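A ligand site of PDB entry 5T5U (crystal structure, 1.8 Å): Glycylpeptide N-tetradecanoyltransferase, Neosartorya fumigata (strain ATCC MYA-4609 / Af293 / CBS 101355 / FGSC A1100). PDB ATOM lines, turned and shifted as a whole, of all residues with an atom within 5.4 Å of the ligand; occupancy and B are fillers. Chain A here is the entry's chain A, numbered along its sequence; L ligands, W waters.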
ATOM      1  N   VAL A  67     -28.135   0.519 -31.930  1.00  0.00           N
ATOM      2  CA  VAL A  67     -27.184   0.926 -30.916  1.00  0.00           C
ATOM      3  C   VAL A  67     -27.705   0.793 -29.472  1.00  0.00           C
ATOM      4  O   VAL A  67     -28.753   1.341 -29.118  1.00  0.00           O
ATOM      5  CB  VAL A  67     -26.738   2.394 -31.150  1.00  0.00           C
ATOM      6  CG1 VAL A  67     -25.729   2.836 -30.130  1.00  0.00           C
ATOM      7  CG2 VAL A  67     -26.222   2.564 -32.577  1.00  0.00           C
ATOM      8  N   GLU A  68     -26.943   0.071 -28.667  1.00  0.00           N
ATOM      9  CA  GLU A  68     -27.145  -0.066 -27.233  1.00  0.00           C
ATOM     10  C   GLU A  68     -26.012   0.623 -26.436  1.00  0.00           C
ATOM     11  O   GLU A  68     -24.951   0.936 -26.981  1.00  0.00           O
ATOM     12  CB  GLU A  68     -27.177  -1.548 -26.851  1.00  0.00           C
ATOM     13  CG  GLU A  68     -28.181  -2.339 -27.618  1.00  0.00           C
ATOM     14  CD  GLU A  68     -28.186  -3.825 -27.261  1.00  0.00           C
ATOM     15  OE1 GLU A  68     -27.461  -4.229 -26.329  1.00  0.00           O
ATOM     16  OE2 GLU A  68     -28.927  -4.579 -27.930  1.00  0.00           O
ATOM     17  N   ASP A  69     -26.239   0.821 -25.145  1.00  0.00           N
ATOM     18  CA  ASP A  69     -25.190   1.301 -24.241  1.00  0.00           C
ATOM     19  C   ASP A  69     -24.272   0.146 -23.932  1.00  0.00           C
ATOM     20  O   ASP A  69     -24.567  -1.001 -24.305  1.00  0.00           O
ATOM     21  CB  ASP A  69     -25.812   1.889 -22.968  1.00  0.00           C
ATOM     22  CG  ASP A  69     -26.436   0.851 -22.080  1.00  0.00           C
ATOM     23  OD1 ASP A  69     -27.407   0.194 -22.502  1.00  0.00           O
ATOM     24  OD2 ASP A  69     -25.967   0.687 -20.925  1.00  0.00           O
ATOM     25  N   PHE A  74     -30.043  -0.110 -22.394  1.00  0.00           N
ATOM     26  CA  PHE A  74     -30.860   0.700 -23.281  1.00  0.00           C
ATOM     27  C   PHE A  74     -30.505   0.453 -24.755  1.00  0.00           C
ATOM     28  O   PHE A  74     -29.340   0.213 -25.091  1.00  0.00           O
ATOM     29  CB  PHE A  74     -30.674   2.192 -22.986  1.00  0.00           C
ATOM     30  CG  PHE A  74     -30.829   2.549 -21.535  1.00  0.00           C
ATOM     31  CD1 PHE A  74     -32.063   2.462 -20.905  1.00  0.00           C
ATOM     32  CD2 PHE A  74     -29.735   2.988 -20.809  1.00  0.00           C
ATOM     33  CE1 PHE A  74     -32.200   2.792 -19.557  1.00  0.00           C
ATOM     34  CE2 PHE A  74     -29.864   3.338 -19.455  1.00  0.00           C
ATOM     35  CZ  PHE A  74     -31.080   3.220 -18.845  1.00  0.00           C
ATOM     36  N   ARG A  75     -31.492   0.586 -25.610  1.00  0.00           N
ATOM     37  CA  ARG A  75     -31.279   0.523 -27.050  1.00  0.00           C
ATOM     38  C   ARG A  75     -32.090   1.644 -27.724  1.00  0.00           C
ATOM     39  O   ARG A  75     -33.275   1.793 -27.444  1.00  0.00           O
ATOM     40  CB  ARG A  75     -31.703  -0.842 -27.605  1.00  0.00           C
ATOM     41  CG  ARG A  75     -31.197  -1.085 -29.015  1.00  0.00           C
ATOM     42  CD  ARG A  75     -31.680  -2.408 -29.564  1.00  0.00           C
ATOM     43  NE  ARG A  75     -31.401  -3.507 -28.677  1.00  0.00           N
ATOM     44  CZ  ARG A  75     -32.332  -4.233 -28.039  1.00  0.00           C
ATOM     45  NH1 ARG A  75     -33.618  -3.978 -28.206  1.00  0.00           N
ATOM     46  NH2 ARG A  75     -31.960  -5.221 -27.237  1.00  0.00           N
ATOM     47  N   PHE A  76     -31.456   2.412 -28.598  1.00  0.00           N
ATOM     48  CA  PHE A  76     -32.199   3.486 -29.279  1.00  0.00           C
ATOM     49  C   PHE A  76     -33.394   2.889 -29.995  1.00  0.00           C
ATOM     50  O   PHE A  76     -33.339   1.779 -30.502  1.00  0.00           O
ATOM     51  CB  PHE A  76     -31.279   4.279 -30.243  1.00  0.00           C
ATOM     52  CG  PHE A  76     -30.260   5.136 -29.549  1.00  0.00           C
ATOM     53  CD1 PHE A  76     -30.652   6.207 -28.745  1.00  0.00           C
ATOM     54  CD2 PHE A  76     -28.903   4.888 -29.653  1.00  0.00           C
ATOM     55  CE1 PHE A  76     -29.708   7.002 -28.111  1.00  0.00           C
ATOM     56  CE2 PHE A  76     -27.969   5.662 -29.035  1.00  0.00           C
ATOM     57  CZ  PHE A  76     -28.362   6.708 -28.248  1.00  0.00           C
ATOM     58  N   TYR A  78     -35.784   4.242 -32.615  1.00  0.00           N
ATOM     59  CA  TYR A  78     -36.310   5.154 -33.624  1.00  0.00           C
ATOM     60  C   TYR A  78     -37.725   4.764 -34.007  1.00  0.00           C
ATOM     61  O   TYR A  78     -37.984   3.584 -34.269  1.00  0.00           O
ATOM     62  CB  TYR A  78     -35.385   5.161 -34.852  1.00  0.00           C
ATOM     63  CG  TYR A  78     -34.062   5.837 -34.644  1.00  0.00           C
ATOM     64  CD1 TYR A  78     -32.988   5.152 -34.090  1.00  0.00           C
ATOM     65  CD2 TYR A  78     -33.900   7.187 -34.982  1.00  0.00           C
ATOM     66  CE1 TYR A  78     -31.761   5.774 -33.887  1.00  0.00           C
ATOM     67  CE2 TYR A  78     -32.697   7.836 -34.799  1.00  0.00           C
ATOM     68  CZ  TYR A  78     -31.629   7.133 -34.231  1.00  0.00           C
ATOM     69  OH  TYR A  78     -30.417   7.740 -34.024  1.00  0.00           O
ATOM     70  N   THR A 168     -21.524  10.035 -38.137  1.00  0.00           N
ATOM     71  CA  THR A 168     -21.014   9.955 -36.765  1.00  0.00           C
ATOM     72  C   THR A 168     -20.928   8.491 -36.357  1.00  0.00           C
ATOM     73  O   THR A 168     -21.607   7.637 -36.942  1.00  0.00           O
ATOM     74  CB  THR A 168     -21.902  10.717 -35.773  1.00  0.00           C
ATOM     75  OG1 THR A 168     -23.202  10.126 -35.730  1.00  0.00           O
ATOM     76  CG2 THR A 168     -22.016  12.216 -36.160  1.00  0.00           C
ATOM     77  N   TYR A 182     -21.566  13.672 -24.937  1.00  0.00           N
ATOM     78  CA  TYR A 182     -22.987  13.615 -24.645  1.00  0.00           C
ATOM     79  C   TYR A 182     -23.324  14.280 -23.304  1.00  0.00           C
ATOM     80  O   TYR A 182     -22.582  14.137 -22.329  1.00  0.00           O
ATOM     81  CB  TYR A 182     -23.476  12.168 -24.539  1.00  0.00           C
ATOM     82  CG  TYR A 182     -23.051  11.248 -25.657  1.00  0.00           C
ATOM     83  CD1 TYR A 182     -23.698  11.253 -26.889  1.00  0.00           C
ATOM     84  CD2 TYR A 182     -22.021  10.353 -25.467  1.00  0.00           C
ATOM     85  CE1 TYR A 182     -23.304  10.385 -27.906  1.00  0.00           C
ATOM     86  CE2 TYR A 182     -21.620   9.467 -26.461  1.00  0.00           C
ATOM     87  CZ  TYR A 182     -22.241   9.508 -27.683  1.00  0.00           C
ATOM     88  OH  TYR A 182     -21.838   8.622 -28.668  1.00  0.00           O
ATOM     89  N   TYR A 183     -24.473  14.939 -23.265  1.00  0.00           N
ATOM     90  CA  TYR A 183     -24.977  15.582 -22.053  1.00  0.00           C
ATOM     91  C   TYR A 183     -26.458  15.294 -21.882  1.00  0.00           C
ATOM     92  O   TYR A 183     -27.195  15.188 -22.856  1.00  0.00           O
ATOM     93  CB  TYR A 183     -24.649  17.081 -22.063  1.00  0.00           C
ATOM     94  CG  TYR A 183     -23.316  17.349 -21.411  1.00  0.00           C
ATOM     95  CD1 TYR A 183     -22.135  17.110 -22.089  1.00  0.00           C
ATOM     96  CD2 TYR A 183     -23.242  17.757 -20.063  1.00  0.00           C
ATOM     97  CE1 TYR A 183     -20.917  17.321 -21.490  1.00  0.00           C
ATOM     98  CE2 TYR A 183     -22.025  17.960 -19.452  1.00  0.00           C
ATOM     99  CZ  TYR A 183     -20.868  17.724 -20.157  1.00  0.00           C
ATOM    100  OH  TYR A 183     -19.664  17.920 -19.543  1.00  0.00           O
ATOM    101  N   HIS A 184     -26.890  15.157 -20.629  1.00  0.00           N
ATOM    102  CA  HIS A 184     -28.223  14.687 -20.308  1.00  0.00           C
ATOM    103  C   HIS A 184     -28.847  15.518 -19.222  1.00  0.00           C
ATOM    104  O   HIS A 184     -28.278  15.618 -18.133  1.00  0.00           O
ATOM    105  CB  HIS A 184     -28.176  13.214 -19.850  1.00  0.00           C
ATOM    106  CG  HIS A 184     -27.231  12.371 -20.616  1.00  0.00           C
ATOM    107  ND1 HIS A 184     -27.383  12.130 -21.962  1.00  0.00           N
ATOM    108  CD2 HIS A 184     -26.104  11.728 -20.243  1.00  0.00           C
ATOM    109  CE1 HIS A 184     -26.382  11.367 -22.390  1.00  0.00           C
ATOM    110  NE2 HIS A 184     -25.606  11.086 -21.351  1.00  0.00           N
ATOM    111  N   PHE A 197     -31.195   4.920 -15.468  1.00  0.00           N
ATOM    112  CA  PHE A 197     -30.570   5.956 -16.264  1.00  0.00           C
ATOM    113  C   PHE A 197     -29.798   6.907 -15.361  1.00  0.00           C
ATOM    114  O   PHE A 197     -28.649   7.204 -15.622  1.00  0.00           O
ATOM    115  CB  PHE A 197     -31.640   6.717 -17.075  1.00  0.00           C
ATOM    116  CG  PHE A 197     -31.082   7.728 -18.050  1.00  0.00           C
ATOM    117  CD1 PHE A 197     -30.629   8.954 -17.605  1.00  0.00           C
ATOM    118  CD2 PHE A 197     -31.021   7.424 -19.397  1.00  0.00           C
ATOM    119  CE1 PHE A 197     -30.119   9.890 -18.499  1.00  0.00           C
ATOM    120  CE2 PHE A 197     -30.510   8.337 -20.298  1.00  0.00           C
ATOM    121  CZ  PHE A 197     -30.059   9.585 -19.856  1.00  0.00           C
ATOM    122  N   TYR A 293     -35.808  17.044 -31.115  1.00  0.00           N
ATOM    123  CA  TYR A 293     -36.549  15.926 -31.673  1.00  0.00           C
ATOM    124  C   TYR A 293     -36.786  14.819 -30.685  1.00  0.00           C
ATOM    125  O   TYR A 293     -36.130  14.739 -29.650  1.00  0.00           O
ATOM    126  CB  TYR A 293     -35.890  15.379 -32.948  1.00  0.00           C
ATOM    127  CG  TYR A 293     -34.464  14.884 -32.827  1.00  0.00           C
ATOM    128  CD1 TYR A 293     -34.189  13.608 -32.337  1.00  0.00           C
ATOM    129  CD2 TYR A 293     -33.406  15.647 -33.279  1.00  0.00           C
ATOM    130  CE1 TYR A 293     -32.876  13.143 -32.260  1.00  0.00           C
ATOM    131  CE2 TYR A 293     -32.100  15.194 -33.202  1.00  0.00           C
ATOM    132  CZ  TYR A 293     -31.842  13.951 -32.692  1.00  0.00           C
ATOM    133  OH  TYR A 293     -30.537  13.528 -32.630  1.00  0.00           O
ATOM    134  N   SER A 297     -35.758   5.496 -26.256  1.00  0.00           N
ATOM    135  CA  SER A 297     -34.906   4.368 -26.031  1.00  0.00           C
ATOM    136  C   SER A 297     -35.709   3.233 -25.393  1.00  0.00           C
ATOM    137  O   SER A 297     -36.538   3.470 -24.505  1.00  0.00           O
ATOM    138  CB  SER A 297     -33.715   4.695 -25.165  1.00  0.00           C
ATOM    139  OG  SER A 297     -32.736   5.433 -25.875  1.00  0.00           O
ATOM    140  N   VAL A 308     -37.631   4.967 -22.401  1.00  0.00           N
ATOM    141  CA  VAL A 308     -37.259   6.324 -22.031  1.00  0.00           C
ATOM    142  C   VAL A 308     -37.700   7.256 -23.172  1.00  0.00           C
ATOM    143  O   VAL A 308     -37.327   7.055 -24.336  1.00  0.00           O
ATOM    144  CB  VAL A 308     -35.731   6.464 -21.790  1.00  0.00           C
ATOM    145  CG1 VAL A 308     -35.343   7.954 -21.584  1.00  0.00           C
ATOM    146  CG2 VAL A 308     -35.314   5.624 -20.605  1.00  0.00           C
ATOM    147  N   TYR A 312     -34.019  15.451 -27.935  1.00  0.00           N
ATOM    148  CA  TYR A 312     -32.675  15.845 -28.289  1.00  0.00           C
ATOM    149  C   TYR A 312     -32.634  17.236 -28.897  1.00  0.00           C
ATOM    150  O   TYR A 312     -33.368  17.530 -29.751  1.00  0.00           O
ATOM    151  CB  TYR A 312     -32.027  14.873 -29.289  1.00  0.00           C
ATOM    152  CG  TYR A 312     -31.839  13.519 -28.750  1.00  0.00           C
ATOM    153  CD1 TYR A 312     -32.923  12.712 -28.452  1.00  0.00           C
ATOM    154  CD2 TYR A 312     -30.606  13.038 -28.512  1.00  0.00           C
ATOM    155  CE1 TYR A 312     -32.754  11.466 -27.945  1.00  0.00           C
ATOM    156  CE2 TYR A 312     -30.410  11.796 -27.990  1.00  0.00           C
ATOM    157  CZ  TYR A 312     -31.476  11.014 -27.699  1.00  0.00           C
ATOM    158  OH  TYR A 312     -31.237   9.777 -27.186  1.00  0.00           O
ATOM    159  N   ASN A 353     -31.618  15.725 -24.110  1.00  0.00           N
ATOM    160  CA  ASN A 353     -30.232  15.405 -24.416  1.00  0.00           C
ATOM    161  C   ASN A 353     -29.553  16.405 -25.351  1.00  0.00           C
ATOM    162  O   ASN A 353     -30.203  17.006 -26.191  1.00  0.00           O
ATOM    163  CB  ASN A 353     -30.158  14.016 -25.043  1.00  0.00           C
ATOM    164  CG  ASN A 353     -30.596  12.935 -24.102  1.00  0.00           C
ATOM    165  OD1 ASN A 353     -30.191  12.906 -22.923  1.00  0.00           O
ATOM    166  ND2 ASN A 353     -31.415  12.042 -24.583  1.00  0.00           N
ATOM    167  N   ALA A 354     -28.254  16.596 -25.186  1.00  0.00           N
ATOM    168  CA  ALA A 354     -27.491  17.458 -26.076  1.00  0.00           C
ATOM    169  C   ALA A 354     -26.042  17.027 -26.184  1.00  0.00           C
ATOM    170  O   ALA A 354     -25.558  16.226 -25.388  1.00  0.00           O
ATOM    171  CB  ALA A 354     -27.613  18.888 -25.590  1.00  0.00           C
ATOM    172  N   LEU A 355     -25.338  17.613 -27.150  1.00  0.00           N
ATOM    173  CA  LEU A 355     -23.932  17.406 -27.393  1.00  0.00           C
ATOM    174  C   LEU A 355     -23.192  18.692 -27.125  1.00  0.00           C
ATOM    175  O   LEU A 355     -23.812  19.750 -26.985  1.00  0.00           O
ATOM    176  CB  LEU A 355     -23.700  16.975 -28.869  1.00  0.00           C
ATOM    177  CG  LEU A 355     -24.324  15.639 -29.245  1.00  0.00           C
ATOM    178  CD1 LEU A 355     -24.395  15.469 -30.739  1.00  0.00           C
ATOM    179  CD2 LEU A 355     -23.580  14.493 -28.596  1.00  0.00           C
ATOM    180  N   LEU A 376     -19.221  11.300 -29.043  1.00  0.00           N
ATOM    181  CA  LEU A 376     -19.648  10.989 -30.398  1.00  0.00           C
ATOM    182  C   LEU A 376     -18.601  11.544 -31.364  1.00  0.00           C
ATOM    183  O   LEU A 376     -18.275  12.731 -31.332  1.00  0.00           O
ATOM    184  CB  LEU A 376     -21.015  11.585 -30.668  1.00  0.00           C
ATOM    185  CG  LEU A 376     -21.549  11.291 -32.066  1.00  0.00           C
ATOM    186  CD1 LEU A 376     -21.787   9.812 -32.230  1.00  0.00           C
ATOM    187  CD2 LEU A 376     -22.800  12.132 -32.309  1.00  0.00           C
ATOM    188  N   MET A 410     -26.522  15.547 -36.350  1.00  0.00           N
ATOM    189  CA  MET A 410     -27.037  14.426 -37.126  1.00  0.00           C
ATOM    190  C   MET A 410     -27.793  13.482 -36.205  1.00  0.00           C
ATOM    191  O   MET A 410     -27.585  13.486 -34.981  1.00  0.00           O
ATOM    192  CB  MET A 410     -25.906  13.714 -37.833  1.00  0.00           C
ATOM    193  CG  MET A 410     -25.046  14.647 -38.681  1.00  0.00           C
ATOM    194  SD  MET A 410     -23.728  13.806 -39.550  1.00  0.00           S
ATOM    195  CE  MET A 410     -24.629  12.663 -40.557  1.00  0.00           C
ATOM    196  N   LEU A 411     -28.643  12.671 -36.814  1.00  0.00           N
ATOM    197  CA  LEU A 411     -29.703  11.980 -36.115  1.00  0.00           C
ATOM    198  C   LEU A 411     -29.264  10.674 -35.446  1.00  0.00           C
ATOM    199  O   LEU A 411     -28.182  10.146 -35.696  1.00  0.00           O
ATOM    200  CB  LEU A 411     -30.811  11.664 -37.101  1.00  0.00           C
ATOM    201  CG  LEU A 411     -31.410  12.952 -37.705  1.00  0.00           C
ATOM    202  CD1 LEU A 411     -32.243  12.618 -38.907  1.00  0.00           C
ATOM    203  CD2 LEU A 411     -32.244  13.633 -36.651  1.00  0.00           C
ATOM    204  OXT LEU A 411     -30.041  10.124 -34.636  1.00  0.00           O
HETATM  205  C1  LIG L   1     -27.579  11.388 -31.296  1.00  0.00           C
HETATM  206  C2  LIG L   1     -27.250  10.973 -32.742  1.00  0.00           C
HETATM  207  N1  LIG L   1     -26.939   9.525 -32.831  1.00  0.00           N
HETATM  208  C3  LIG L   1     -25.816   9.200 -31.955  1.00  0.00           C
HETATM  209  C4  LIG L   1     -26.180   9.519 -30.511  1.00  0.00           C
HETATM  210  C5  LIG L   1     -26.419  11.017 -30.422  1.00  0.00           C
HETATM  211  C6  LIG L   1     -26.722  11.421 -28.990  1.00  0.00           C
HETATM  212  C7  LIG L   1     -26.885  10.434 -28.023  1.00  0.00           C
HETATM  213  C8  LIG L   1     -26.872  12.776 -28.662  1.00  0.00           C
HETATM  214  C9  LIG L   1     -27.145  13.133 -27.353  1.00  0.00           C
HETATM  215  C10 LIG L   1     -27.296  12.153 -26.389  1.00  0.00           C
HETATM  216  C11 LIG L   1     -27.204  10.792 -26.736  1.00  0.00           C
HETATM  217  C12 LIG L   1     -27.381   9.847 -25.751  1.00  0.00           C
HETATM  218  C13 LIG L   1     -26.641   8.666 -25.713  1.00  0.00           C
HETATM  219  C14 LIG L   1     -26.843   7.791 -24.630  1.00  0.00           C
HETATM  220  C15 LIG L   1     -28.262  10.152 -24.719  1.00  0.00           C
HETATM  221  C16 LIG L   1     -28.462   9.269 -23.676  1.00  0.00           C
HETATM  222  C17 LIG L   1     -27.749   8.066 -23.630  1.00  0.00           C
HETATM  223  O1  LIG L   1     -27.958   7.211 -22.569  1.00  0.00           O
HETATM  224  C18 LIG L   1     -27.692   5.818 -22.893  1.00  0.00           C
HETATM  225  C19 LIG L   1     -28.325   5.224 -23.975  1.00  0.00           C
HETATM  226  C20 LIG L   1     -27.547   4.582 -24.931  1.00  0.00           C
HETATM  227  C21 LIG L   1     -28.200   3.994 -26.020  1.00  0.00           C
HETATM  228  C22 LIG L   1     -29.562   4.080 -26.139  1.00  0.00           C
HETATM  229  N2  LIG L   1     -30.302   4.723 -25.220  1.00  0.00           N
HETATM  230  C23 LIG L   1     -29.723   5.291 -24.146  1.00  0.00           C
HETATM  231  C24 LIG L   1     -30.632   5.958 -23.126  1.00  0.00           C
HETATM  232  O   HOH W   1     -24.358   4.924 -23.220  1.00  0.00           O
HETATM  233  O   HOH W   2     -23.496   7.166 -24.513  1.00  0.00           O
HETATM  234  O   HOH W   3     -24.186   7.084 -29.444  1.00  0.00           O
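OG of Ser 297 is in hydrogen-bond range of N2 of the ligand (2.6 Å). The chain-end carboxylate (O) of Leu 411 lies within salt-bridge range of a nitrogen (N1) of the ligand.
The chain-end carboxylate (OXT) of Leu 411 is in hydrogen-bond range of the side-chain hydroxyl (OH) of Tyr 78, 2.5 Å away. ND1 of His 184 is in hydrogen-bond range of OD1 of Asn 353 (3.1 Å). N of Phe 74 lies within hydrogen-bond range of OD1 of Asp 69. The backbone NH (N) of Phe 76 sits at hydrogen-bond distance from the backbone carbonyl oxygen (O) of Val 67, at 3.0 Å. OH of Tyr 312 sits close to ND2 of Asn 353 (3.5 Å). The backbone carbonyl oxygen (O) of Tyr 293 lies within hydrogen-bond range of the backbone NH (N) of Tyr 312 (2.8 Å). OE2 of Glu 68 lies within salt-bridge range of NE of Arg 75 (2.8 Å). O of Ala 354 lies within hydrogen-bond range of N of Tyr 183 (2.7 Å).
CB of Asp 69 touches C20 of the ligand, 3.8 Å away. Phe 74 touches the ligand. Arg 75 touches the ligand (C to C22, 3.9 Å). Phe 76 touches the ligand. Tyr 182 touches the ligand. His 184 touches the ligand. Phe 197 touches the ligand. OH of Tyr 293 touches C1 of the ligand, 3.9 Å away. CE2 of Tyr 312 touches C10 of the ligand, at 3.5 Å. Asn 353 touches the ligand. Ala 354 touches the ligand. Leu 355 touches the ligand (CD2 to C8, 3.7 Å). Met 410 touches the ligand (O to C2, 3.4 Å). Hydrophobic or aromatic side chains within 4 Å of the ligand: Phe 74, Phe 76, Tyr 182, His 184, Phe 197, Tyr 312 and Leu 355. Of the 22 residues printed, 15 come within 4 Å of the ligand.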
